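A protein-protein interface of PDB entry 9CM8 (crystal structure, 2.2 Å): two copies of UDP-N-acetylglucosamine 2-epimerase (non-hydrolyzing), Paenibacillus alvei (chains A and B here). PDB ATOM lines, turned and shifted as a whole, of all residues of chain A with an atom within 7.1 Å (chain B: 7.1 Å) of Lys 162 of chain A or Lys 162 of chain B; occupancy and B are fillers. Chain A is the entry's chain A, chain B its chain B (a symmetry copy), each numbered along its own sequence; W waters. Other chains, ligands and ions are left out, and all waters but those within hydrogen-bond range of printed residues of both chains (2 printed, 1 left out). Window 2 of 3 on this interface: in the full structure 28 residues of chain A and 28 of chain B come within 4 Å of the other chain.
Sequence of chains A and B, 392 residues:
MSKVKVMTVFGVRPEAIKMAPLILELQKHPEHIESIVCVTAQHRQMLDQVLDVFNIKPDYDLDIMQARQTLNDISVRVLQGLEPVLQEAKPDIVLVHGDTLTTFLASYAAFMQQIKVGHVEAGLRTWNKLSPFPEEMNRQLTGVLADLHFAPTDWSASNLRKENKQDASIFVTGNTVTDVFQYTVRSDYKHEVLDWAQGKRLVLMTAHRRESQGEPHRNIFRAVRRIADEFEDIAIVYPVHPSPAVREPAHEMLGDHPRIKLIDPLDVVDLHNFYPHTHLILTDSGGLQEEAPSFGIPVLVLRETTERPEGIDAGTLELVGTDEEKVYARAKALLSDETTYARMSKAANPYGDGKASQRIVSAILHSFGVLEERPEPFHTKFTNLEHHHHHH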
ATOM      1  N   TRP A 127     -36.125  -1.670   7.490  1.00  0.00           N
ATOM      2  CA  TRP A 127     -35.154  -1.349   6.408  1.00  0.00           C
ATOM      3  C   TRP A 127     -35.720  -0.260   5.466  1.00  0.00           C
ATOM      4  O   TRP A 127     -35.325  -0.242   4.297  1.00  0.00           O
ATOM      5  CB  TRP A 127     -34.732  -2.629   5.662  1.00  0.00           C
ATOM      6  CG  TRP A 127     -34.339  -3.772   6.551  1.00  0.00           C
ATOM      7  CD1 TRP A 127     -35.081  -4.891   6.826  1.00  0.00           C
ATOM      8  CD2 TRP A 127     -33.104  -3.935   7.275  1.00  0.00           C
ATOM      9  NE1 TRP A 127     -34.390  -5.733   7.666  1.00  0.00           N
ATOM     10  CE2 TRP A 127     -33.178  -5.173   7.961  1.00  0.00           C
ATOM     11  CE3 TRP A 127     -31.949  -3.163   7.423  1.00  0.00           C
ATOM     12  CZ2 TRP A 127     -32.152  -5.647   8.776  1.00  0.00           C
ATOM     13  CZ3 TRP A 127     -30.926  -3.632   8.228  1.00  0.00           C
ATOM     14  CH2 TRP A 127     -31.026  -4.863   8.888  1.00  0.00           C
ATOM     15  N   TRP A 155     -35.373 -12.654  16.341  1.00  0.00           N
ATOM     16  CA  TRP A 155     -35.551 -11.908  15.062  1.00  0.00           C
ATOM     17  C   TRP A 155     -34.770 -10.576  15.122  1.00  0.00           C
ATOM     18  O   TRP A 155     -33.996 -10.322  14.215  1.00  0.00           O
ATOM     19  CB  TRP A 155     -37.027 -11.689  14.742  1.00  0.00           C
ATOM     20  CG  TRP A 155     -37.249 -10.900  13.488  1.00  0.00           C
ATOM     21  CD1 TRP A 155     -37.189 -11.365  12.207  1.00  0.00           C
ATOM     22  CD2 TRP A 155     -37.580  -9.497  13.393  1.00  0.00           C
ATOM     23  NE1 TRP A 155     -37.480 -10.358  11.327  1.00  0.00           N
ATOM     24  CE2 TRP A 155     -37.738  -9.205  12.021  1.00  0.00           C
ATOM     25  CE3 TRP A 155     -37.781  -8.476  14.330  1.00  0.00           C
ATOM     26  CZ2 TRP A 155     -38.059  -7.928  11.554  1.00  0.00           C
ATOM     27  CZ3 TRP A 155     -38.083  -7.208  13.871  1.00  0.00           C
ATOM     28  CH2 TRP A 155     -38.226  -6.940  12.499  1.00  0.00           C
ATOM     29  N   ALA A 157     -32.148  -9.926  17.089  1.00  0.00           N
ATOM     30  CA  ALA A 157     -30.705 -10.246  17.124  1.00  0.00           C
ATOM     31  C   ALA A 157     -30.232 -10.554  15.699  1.00  0.00           C
ATOM     32  O   ALA A 157     -29.144 -10.078  15.312  1.00  0.00           O
ATOM     33  CB  ALA A 157     -30.422 -11.394  18.047  1.00  0.00           C
ATOM     34  N   SER A 158     -31.027 -11.283  14.920  1.00  0.00           N
ATOM     35  CA  SER A 158     -30.639 -11.622  13.527  1.00  0.00           C
ATOM     36  C   SER A 158     -30.664 -10.360  12.636  1.00  0.00           C
ATOM     37  O   SER A 158     -29.780 -10.225  11.766  1.00  0.00           O
ATOM     38  CB  SER A 158     -31.454 -12.773  12.996  1.00  0.00           C
ATOM     39  OG  SER A 158     -32.654 -12.324  12.403  1.00  0.00           O
ATOM     40  N   ASN A 159     -31.537  -9.383  12.884  1.00  0.00           N
ATOM     41  CA  ASN A 159     -31.396  -8.070  12.182  1.00  0.00           C
ATOM     42  C   ASN A 159     -29.994  -7.517  12.429  1.00  0.00           C
ATOM     43  O   ASN A 159     -29.334  -7.089  11.460  1.00  0.00           O
ATOM     44  CB  ASN A 159     -32.487  -7.078  12.588  1.00  0.00           C
ATOM     45  CG  ASN A 159     -33.851  -7.556  12.152  1.00  0.00           C
ATOM     46  OD1 ASN A 159     -33.962  -8.374  11.226  1.00  0.00           O
ATOM     47  ND2 ASN A 159     -34.890  -7.048  12.792  1.00  0.00           N
ATOM     48  N   LEU A 160     -29.527  -7.565  13.681  1.00  0.00           N
ATOM     49  CA  LEU A 160     -28.203  -7.014  14.069  1.00  0.00           C
ATOM     50  C   LEU A 160     -27.068  -7.814  13.412  1.00  0.00           C
ATOM     51  O   LEU A 160     -26.070  -7.180  12.989  1.00  0.00           O
ATOM     52  CB  LEU A 160     -28.089  -6.969  15.596  1.00  0.00           C
ATOM     53  CG  LEU A 160     -29.004  -5.962  16.290  1.00  0.00           C
ATOM     54  CD1 LEU A 160     -29.028  -6.204  17.785  1.00  0.00           C
ATOM     55  CD2 LEU A 160     -28.551  -4.541  15.987  1.00  0.00           C
ATOM     56  N   ARG A 161     -27.189  -9.144  13.311  1.00  0.00           N
ATOM     57  CA  ARG A 161     -26.185 -10.014  12.625  1.00  0.00           C
ATOM     58  C   ARG A 161     -26.175  -9.664  11.121  1.00  0.00           C
ATOM     59  O   ARG A 161     -25.102  -9.536  10.564  1.00  0.00           O
ATOM     60  CB  ARG A 161     -26.424 -11.506  12.930  1.00  0.00           C
ATOM     61  CG  ARG A 161     -26.218 -11.861  14.397  1.00  0.00           C
ATOM     62  CD  ARG A 161     -26.649 -13.253  14.861  1.00  0.00           C
ATOM     63  NE  ARG A 161     -26.440 -13.431  16.312  1.00  0.00           N
ATOM     64  CZ  ARG A 161     -27.326 -13.902  17.209  1.00  0.00           C
ATOM     65  NH1 ARG A 161     -26.992 -13.976  18.493  1.00  0.00           N
ATOM     66  NH2 ARG A 161     -28.537 -14.289  16.836  1.00  0.00           N
ATOM     67  N   LYS A 162     -27.319  -9.406  10.513  1.00  0.00           N
ATOM     68  CA  LYS A 162     -27.416  -8.979   9.099  1.00  0.00           C
ATOM     69  C   LYS A 162     -26.587  -7.713   8.835  1.00  0.00           C
ATOM     70  O   LYS A 162     -26.263  -7.494   7.685  1.00  0.00           O
ATOM     71  CB  LYS A 162     -28.872  -8.711   8.713  1.00  0.00           C
ATOM     72  CG  LYS A 162     -29.555  -9.848   7.959  1.00  0.00           C
ATOM     73  CD  LYS A 162     -30.982  -9.523   7.561  1.00  0.00           C
ATOM     74  CE  LYS A 162     -31.768 -10.716   7.061  1.00  0.00           C
ATOM     75  NZ  LYS A 162     -32.084 -11.653   8.167  1.00  0.00           N
ATOM     76  N   GLU A 163     -26.324  -6.896   9.870  1.00  0.00           N
ATOM     77  CA  GLU A 163     -25.632  -5.590   9.790  1.00  0.00           C
ATOM     78  C   GLU A 163     -24.179  -5.785  10.220  1.00  0.00           C
ATOM     79  O   GLU A 163     -23.469  -4.799  10.259  1.00  0.00           O
ATOM     80  CB  GLU A 163     -26.300  -4.553  10.703  1.00  0.00           C
ATOM     81  CG  GLU A 163     -27.685  -4.144  10.264  1.00  0.00           C
ATOM     82  CD  GLU A 163     -28.361  -3.081  11.124  1.00  0.00           C
ATOM     83  OE1 GLU A 163     -29.167  -2.306  10.576  1.00  0.00           O
ATOM     84  OE2 GLU A 163     -28.077  -3.021  12.345  1.00  0.00           O
ATOM     85  N   ASN A 164     -23.764  -7.030  10.485  1.00  0.00           N
ATOM     86  CA  ASN A 164     -22.374  -7.401  10.843  1.00  0.00           C
ATOM     87  C   ASN A 164     -22.025  -6.939  12.259  1.00  0.00           C
ATOM     88  O   ASN A 164     -20.847  -6.614  12.496  1.00  0.00           O
ATOM     89  CB  ASN A 164     -21.335  -6.853   9.866  1.00  0.00           C
ATOM     90  CG  ASN A 164     -20.074  -7.690   9.840  1.00  0.00           C
ATOM     91  OD1 ASN A 164     -20.167  -8.888   9.988  1.00  0.00           O
ATOM     92  ND2 ASN A 164     -18.906  -7.093   9.644  1.00  0.00           N
ATOM     93  N   LYS A 165     -22.973  -6.888  13.178  1.00  0.00           N
ATOM     94  CA  LYS A 165     -22.614  -6.636  14.602  1.00  0.00           C
ATOM     95  C   LYS A 165     -21.950  -7.901  15.158  1.00  0.00           C
ATOM     96  O   LYS A 165     -22.411  -8.991  14.789  1.00  0.00           O
ATOM     97  CB  LYS A 165     -23.832  -6.334  15.466  1.00  0.00           C
ATOM     98  CG  LYS A 165     -24.184  -4.868  15.586  1.00  0.00           C
ATOM     99  CD  LYS A 165     -24.533  -4.226  14.319  1.00  0.00           C
ATOM    100  CE  LYS A 165     -24.852  -2.772  14.524  1.00  0.00           C
ATOM    101  NZ  LYS A 165     -25.082  -2.109  13.226  1.00  0.00           N
ATOM    102  N   ILE A 170     -24.234  -8.878  21.342  1.00  0.00           N
ATOM    103  CA  ILE A 170     -25.716  -9.078  21.308  1.00  0.00           C
ATOM    104  C   ILE A 170     -26.169 -10.017  22.441  1.00  0.00           C
ATOM    105  O   ILE A 170     -25.687 -11.143  22.520  1.00  0.00           O
ATOM    106  CB  ILE A 170     -26.146  -9.621  19.929  1.00  0.00           C
ATOM    107  CG1 ILE A 170     -25.538  -8.768  18.805  1.00  0.00           C
ATOM    108  CG2 ILE A 170     -27.662  -9.720  19.840  1.00  0.00           C
ATOM    109  CD1 ILE A 170     -25.914  -9.168  17.409  1.00  0.00           C
ATOM    110  N   TRP B 127     -13.640  -2.699  11.211  1.00  0.00           N
ATOM    111  CA  TRP B 127     -14.605  -3.309  12.159  1.00  0.00           C
ATOM    112  C   TRP B 127     -14.039  -3.221  13.588  1.00  0.00           C
ATOM    113  O   TRP B 127     -14.341  -4.099  14.395  1.00  0.00           O
ATOM    114  CB  TRP B 127     -14.914  -4.753  11.765  1.00  0.00           C
ATOM    115  CG  TRP B 127     -15.158  -4.975  10.303  1.00  0.00           C
ATOM    116  CD1 TRP B 127     -14.308  -5.544   9.397  1.00  0.00           C
ATOM    117  CD2 TRP B 127     -16.367  -4.674   9.586  1.00  0.00           C
ATOM    118  NE1 TRP B 127     -14.898  -5.597   8.163  1.00  0.00           N
ATOM    119  CE2 TRP B 127     -16.171  -5.100   8.252  1.00  0.00           C
ATOM    120  CE3 TRP B 127     -17.585  -4.088   9.940  1.00  0.00           C
ATOM    121  CZ2 TRP B 127     -17.150  -4.947   7.272  1.00  0.00           C
ATOM    122  CZ3 TRP B 127     -18.552  -3.936   8.970  1.00  0.00           C
ATOM    123  CH2 TRP B 127     -18.332  -4.361   7.652  1.00  0.00           C
ATOM    124  N   TRP B 155     -13.976  -4.431  -2.816  1.00  0.00           N
ATOM    125  CA  TRP B 155     -13.770  -4.796  -1.387  1.00  0.00           C
ATOM    126  C   TRP B 155     -14.617  -3.843  -0.519  1.00  0.00           C
ATOM    127  O   TRP B 155     -15.351  -4.319   0.337  1.00  0.00           O
ATOM    128  CB  TRP B 155     -12.282  -4.749  -1.007  1.00  0.00           C
ATOM    129  CG  TRP B 155     -12.052  -5.047   0.444  1.00  0.00           C
ATOM    130  CD1 TRP B 155     -12.131  -6.267   1.060  1.00  0.00           C
ATOM    131  CD2 TRP B 155     -11.730  -4.097   1.479  1.00  0.00           C
ATOM    132  NE1 TRP B 155     -11.900  -6.135   2.408  1.00  0.00           N
ATOM    133  CE2 TRP B 155     -11.624  -4.819   2.687  1.00  0.00           C
ATOM    134  CE3 TRP B 155     -11.560  -2.709   1.506  1.00  0.00           C
ATOM    135  CZ2 TRP B 155     -11.360  -4.197   3.907  1.00  0.00           C
ATOM    136  CZ3 TRP B 155     -11.269  -2.095   2.705  1.00  0.00           C
ATOM    137  CH2 TRP B 155     -11.178  -2.828   3.897  1.00  0.00           C
ATOM    138  N   ALA B 157     -17.311  -1.972  -1.425  1.00  0.00           N
ATOM    139  CA  ALA B 157     -18.706  -2.384  -1.698  1.00  0.00           C
ATOM    140  C   ALA B 157     -19.077  -3.655  -0.916  1.00  0.00           C
ATOM    141  O   ALA B 157     -20.222  -3.717  -0.400  1.00  0.00           O
ATOM    142  CB  ALA B 157     -18.900  -2.579  -3.181  1.00  0.00           C
ATOM    143  N   SER B 158     -18.186  -4.651  -0.843  1.00  0.00           N
ATOM    144  CA  SER B 158     -18.426  -5.909  -0.069  1.00  0.00           C
ATOM    145  C   SER B 158     -18.610  -5.582   1.417  1.00  0.00           C
ATOM    146  O   SER B 158     -19.494  -6.144   2.009  1.00  0.00           O
ATOM    147  CB  SER B 158     -17.326  -6.920  -0.243  1.00  0.00           C
ATOM    148  OG  SER B 158     -17.419  -7.484  -1.535  1.00  0.00           O
ATOM    149  N   ASN B 159     -17.800  -4.693   1.998  1.00  0.00           N
ATOM    150  CA  ASN B 159     -18.024  -4.213   3.399  1.00  0.00           C
ATOM    151  C   ASN B 159     -19.466  -3.701   3.556  1.00  0.00           C
ATOM    152  O   ASN B 159     -20.150  -4.142   4.471  1.00  0.00           O
ATOM    153  CB  ASN B 159     -16.963  -3.178   3.777  1.00  0.00           C
ATOM    154  CG  ASN B 159     -15.560  -3.777   3.759  1.00  0.00           C
ATOM    155  OD1 ASN B 159     -15.418  -4.985   3.847  1.00  0.00           O
ATOM    156  ND2 ASN B 159     -14.530  -2.958   3.659  1.00  0.00           N
ATOM    157  N   LEU B 160     -19.935  -2.843   2.652  1.00  0.00           N
ATOM    158  CA  LEU B 160     -21.284  -2.232   2.708  1.00  0.00           C
ATOM    159  C   LEU B 160     -22.363  -3.325   2.608  1.00  0.00           C
ATOM    160  O   LEU B 160     -23.316  -3.310   3.452  1.00  0.00           O
ATOM    161  CB  LEU B 160     -21.384  -1.175   1.613  1.00  0.00           C
ATOM    162  CG  LEU B 160     -20.440   0.027   1.803  1.00  0.00           C
ATOM    163  CD1 LEU B 160     -20.503   1.012   0.638  1.00  0.00           C
ATOM    164  CD2 LEU B 160     -20.779   0.748   3.114  1.00  0.00           C
ATOM    165  N   ARG B 161     -22.215  -4.302   1.708  1.00  0.00           N
ATOM    166  CA  ARG B 161     -23.159  -5.452   1.622  1.00  0.00           C
ATOM    167  C   ARG B 161     -23.148  -6.256   2.934  1.00  0.00           C
ATOM    168  O   ARG B 161     -24.218  -6.623   3.383  1.00  0.00           O
ATOM    169  CB  ARG B 161     -22.825  -6.372   0.431  1.00  0.00           C
ATOM    170  CG  ARG B 161     -23.000  -5.692  -0.915  1.00  0.00           C
ATOM    171  CD  ARG B 161     -22.907  -6.589  -2.146  1.00  0.00           C
ATOM    172  NE  ARG B 161     -22.937  -5.689  -3.290  1.00  0.00           N
ATOM    173  CZ  ARG B 161     -21.875  -5.266  -3.996  1.00  0.00           C
ATOM    174  NH1 ARG B 161     -20.660  -5.734  -3.758  1.00  0.00           N
ATOM    175  NH2 ARG B 161     -22.049  -4.366  -4.961  1.00  0.00           N
ATOM    176  N   LYS B 162     -21.999  -6.528   3.538  1.00  0.00           N
ATOM    177  CA  LYS B 162     -21.936  -7.159   4.883  1.00  0.00           C
ATOM    178  C   LYS B 162     -22.797  -6.405   5.908  1.00  0.00           C
ATOM    179  O   LYS B 162     -23.125  -7.010   6.941  1.00  0.00           O
ATOM    180  CB  LYS B 162     -20.502  -7.185   5.416  1.00  0.00           C
ATOM    181  CG  LYS B 162     -19.741  -8.474   5.148  1.00  0.00           C
ATOM    182  CD  LYS B 162     -18.363  -8.507   5.793  1.00  0.00           C
ATOM    183  CE  LYS B 162     -17.365  -9.406   5.090  1.00  0.00           C
ATOM    184  NZ  LYS B 162     -16.853  -8.770   3.853  1.00  0.00           N
ATOM    185  N   GLU B 163     -23.092  -5.119   5.676  1.00  0.00           N
ATOM    186  CA  GLU B 163     -23.860  -4.270   6.621  1.00  0.00           C
ATOM    187  C   GLU B 163     -25.311  -4.201   6.152  1.00  0.00           C
ATOM    188  O   GLU B 163     -26.093  -3.459   6.765  1.00  0.00           O
ATOM    189  CB  GLU B 163     -23.213  -2.889   6.753  1.00  0.00           C
ATOM    190  CG  GLU B 163     -21.907  -2.881   7.530  1.00  0.00           C
ATOM    191  CD  GLU B 163     -21.222  -1.522   7.572  1.00  0.00           C
ATOM    192  OE1 GLU B 163     -21.599  -0.620   6.767  1.00  0.00           O
ATOM    193  OE2 GLU B 163     -20.316  -1.346   8.399  1.00  0.00           O
ATOM    194  N   ASN B 164     -25.671  -4.990   5.136  1.00  0.00           N
ATOM    195  CA  ASN B 164     -27.051  -5.075   4.614  1.00  0.00           C
ATOM    196  C   ASN B 164     -27.425  -3.774   3.896  1.00  0.00           C
ATOM    197  O   ASN B 164     -28.610  -3.472   3.846  1.00  0.00           O
ATOM    198  CB  ASN B 164     -28.050  -5.395   5.734  1.00  0.00           C
ATOM    199  CG  ASN B 164     -29.327  -6.016   5.206  1.00  0.00           C
ATOM    200  OD1 ASN B 164     -29.275  -6.848   4.319  1.00  0.00           O
ATOM    201  ND2 ASN B 164     -30.469  -5.633   5.749  1.00  0.00           N
ATOM    202  N   LYS B 165     -26.470  -3.029   3.352  1.00  0.00           N
ATOM    203  CA  LYS B 165     -26.816  -1.907   2.434  1.00  0.00           C
ATOM    204  C   LYS B 165     -27.448  -2.485   1.160  1.00  0.00           C
ATOM    205  O   LYS B 165     -26.976  -3.535   0.690  1.00  0.00           O
ATOM    206  CB  LYS B 165     -25.590  -1.072   2.065  1.00  0.00           C
ATOM    207  CG  LYS B 165     -25.299   0.074   3.014  1.00  0.00           C
ATOM    208  CD  LYS B 165     -24.780  -0.334   4.329  1.00  0.00           C
ATOM    209  CE  LYS B 165     -24.534   0.878   5.194  1.00  0.00           C
ATOM    210  NZ  LYS B 165     -24.174   0.479   6.570  1.00  0.00           N
ATOM    211  N   ILE B 170     -25.300   1.061  -3.950  1.00  0.00           N
ATOM    212  CA  ILE B 170     -23.808   0.968  -3.988  1.00  0.00           C
ATOM    213  C   ILE B 170     -23.330   1.131  -5.433  1.00  0.00           C
ATOM    214  O   ILE B 170     -23.771   0.366  -6.287  1.00  0.00           O
ATOM    215  CB  ILE B 170     -23.283  -0.347  -3.353  1.00  0.00           C
ATOM    216  CG1 ILE B 170     -23.872  -0.594  -1.957  1.00  0.00           C
ATOM    217  CG2 ILE B 170     -21.773  -0.337  -3.319  1.00  0.00           C
ATOM    218  CD1 ILE B 170     -23.644  -1.993  -1.407  1.00  0.00           C
HETATM  219  O   HOH W   1     -33.136  -6.938   5.095  1.00  0.00           O
HETATM  220  O   HOH W   2     -16.366  -8.612   8.933  1.00  0.00           O
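OE2 of Glu 163 of chain A lies within salt-bridge range of NZ of Lys 165 of chain A (3.3 Å). OE1 of Glu 163 of chain B is in salt-bridge range of NZ of Lys 165 of chain B (2.8 Å).
O of Lys 162 of chain A lies close to O of Lys 162 of chain B (3.3 Å).
Of the printed residues of chain B, Trp 127 of chain A touches Asn 164. Ser 158 of chain A touches none of the printed residues of chain B. Of chain B, only Lys 162 (3.3 Å), Glu 163 (3.8 Å) and Asn 164 (3.4 Å) come within 4 Å of Lys 162 of chain A. Of the printed residues of chain A, Trp 127 of chain B touches Asn 164 (3.2 Å). Lys 162 of chain B touches just these residues of chain A: Lys 162, Glu 163 and Asn 164. Printed residues of chain A within 4 Å of Glu 163 of chain B: Lys 162 (3.8 Å) and Glu 163 (3.7 Å). The nearest residue of chain B that does not touch Lys 162 of chain A is Arg 161 of chain B (4.8 Å). The nearest residue of chain A that does not touch Lys 162 of chain B is Arg 161 of chain A (4.8 Å).
Water W1 lies within hydrogen-bond range of the side-chain amide nitrogen of Asn 164 of chain B (3.0 Å) and the indole nitrogen of Trp 127 of chain A (3.1 Å). Water W2 lies within hydrogen-bond range of ND2 of Asn 164 of chain A (3.0 Å) and NE1 of Trp 127 of chain B (3.4 Å).
Lys 162 of chain B touches its own counterpart, Lys 162 of chain A. Lys 162 of chain A touches Glu 163 of chain B, and with the chains exchanged Glu 163 of chain A touches Lys 162 of chain B. Lys 162 of chain A touches Asn 164 of chain B, and with the chains exchanged Asn 164 of chain A touches Lys 162 of chain B. Glu 163 of chain A touches its own counterpart, Glu 163 of chain B.
Hydrophobic or aromatic side chains of chain A within 4 Å of the printed part of chain B: Trp 127. Hydrophobic or aromatic side chains of chain B that line the printed part of chain A: Trp 127.
Among the printed residues, merely in contact across the chains: Trp 127 of chain A with Asn 164 of chain B (3.2 Å), Lys 162 of chain A with Glu 163 of chain B (3.8 Å), Lys 162 of chain A with Asn 164 of chain B (3.4 Å), Glu 163 of chain A with Lys 162 of chain B (3.7 Å), Glu 163 of chain A with Glu 163 of chain B (3.7 Å), Asn 164 of chain A with Trp 127 of chain B (3.2 Å) and Asn 164 of chain A with Lys 162 of chain B (3.4 Å).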
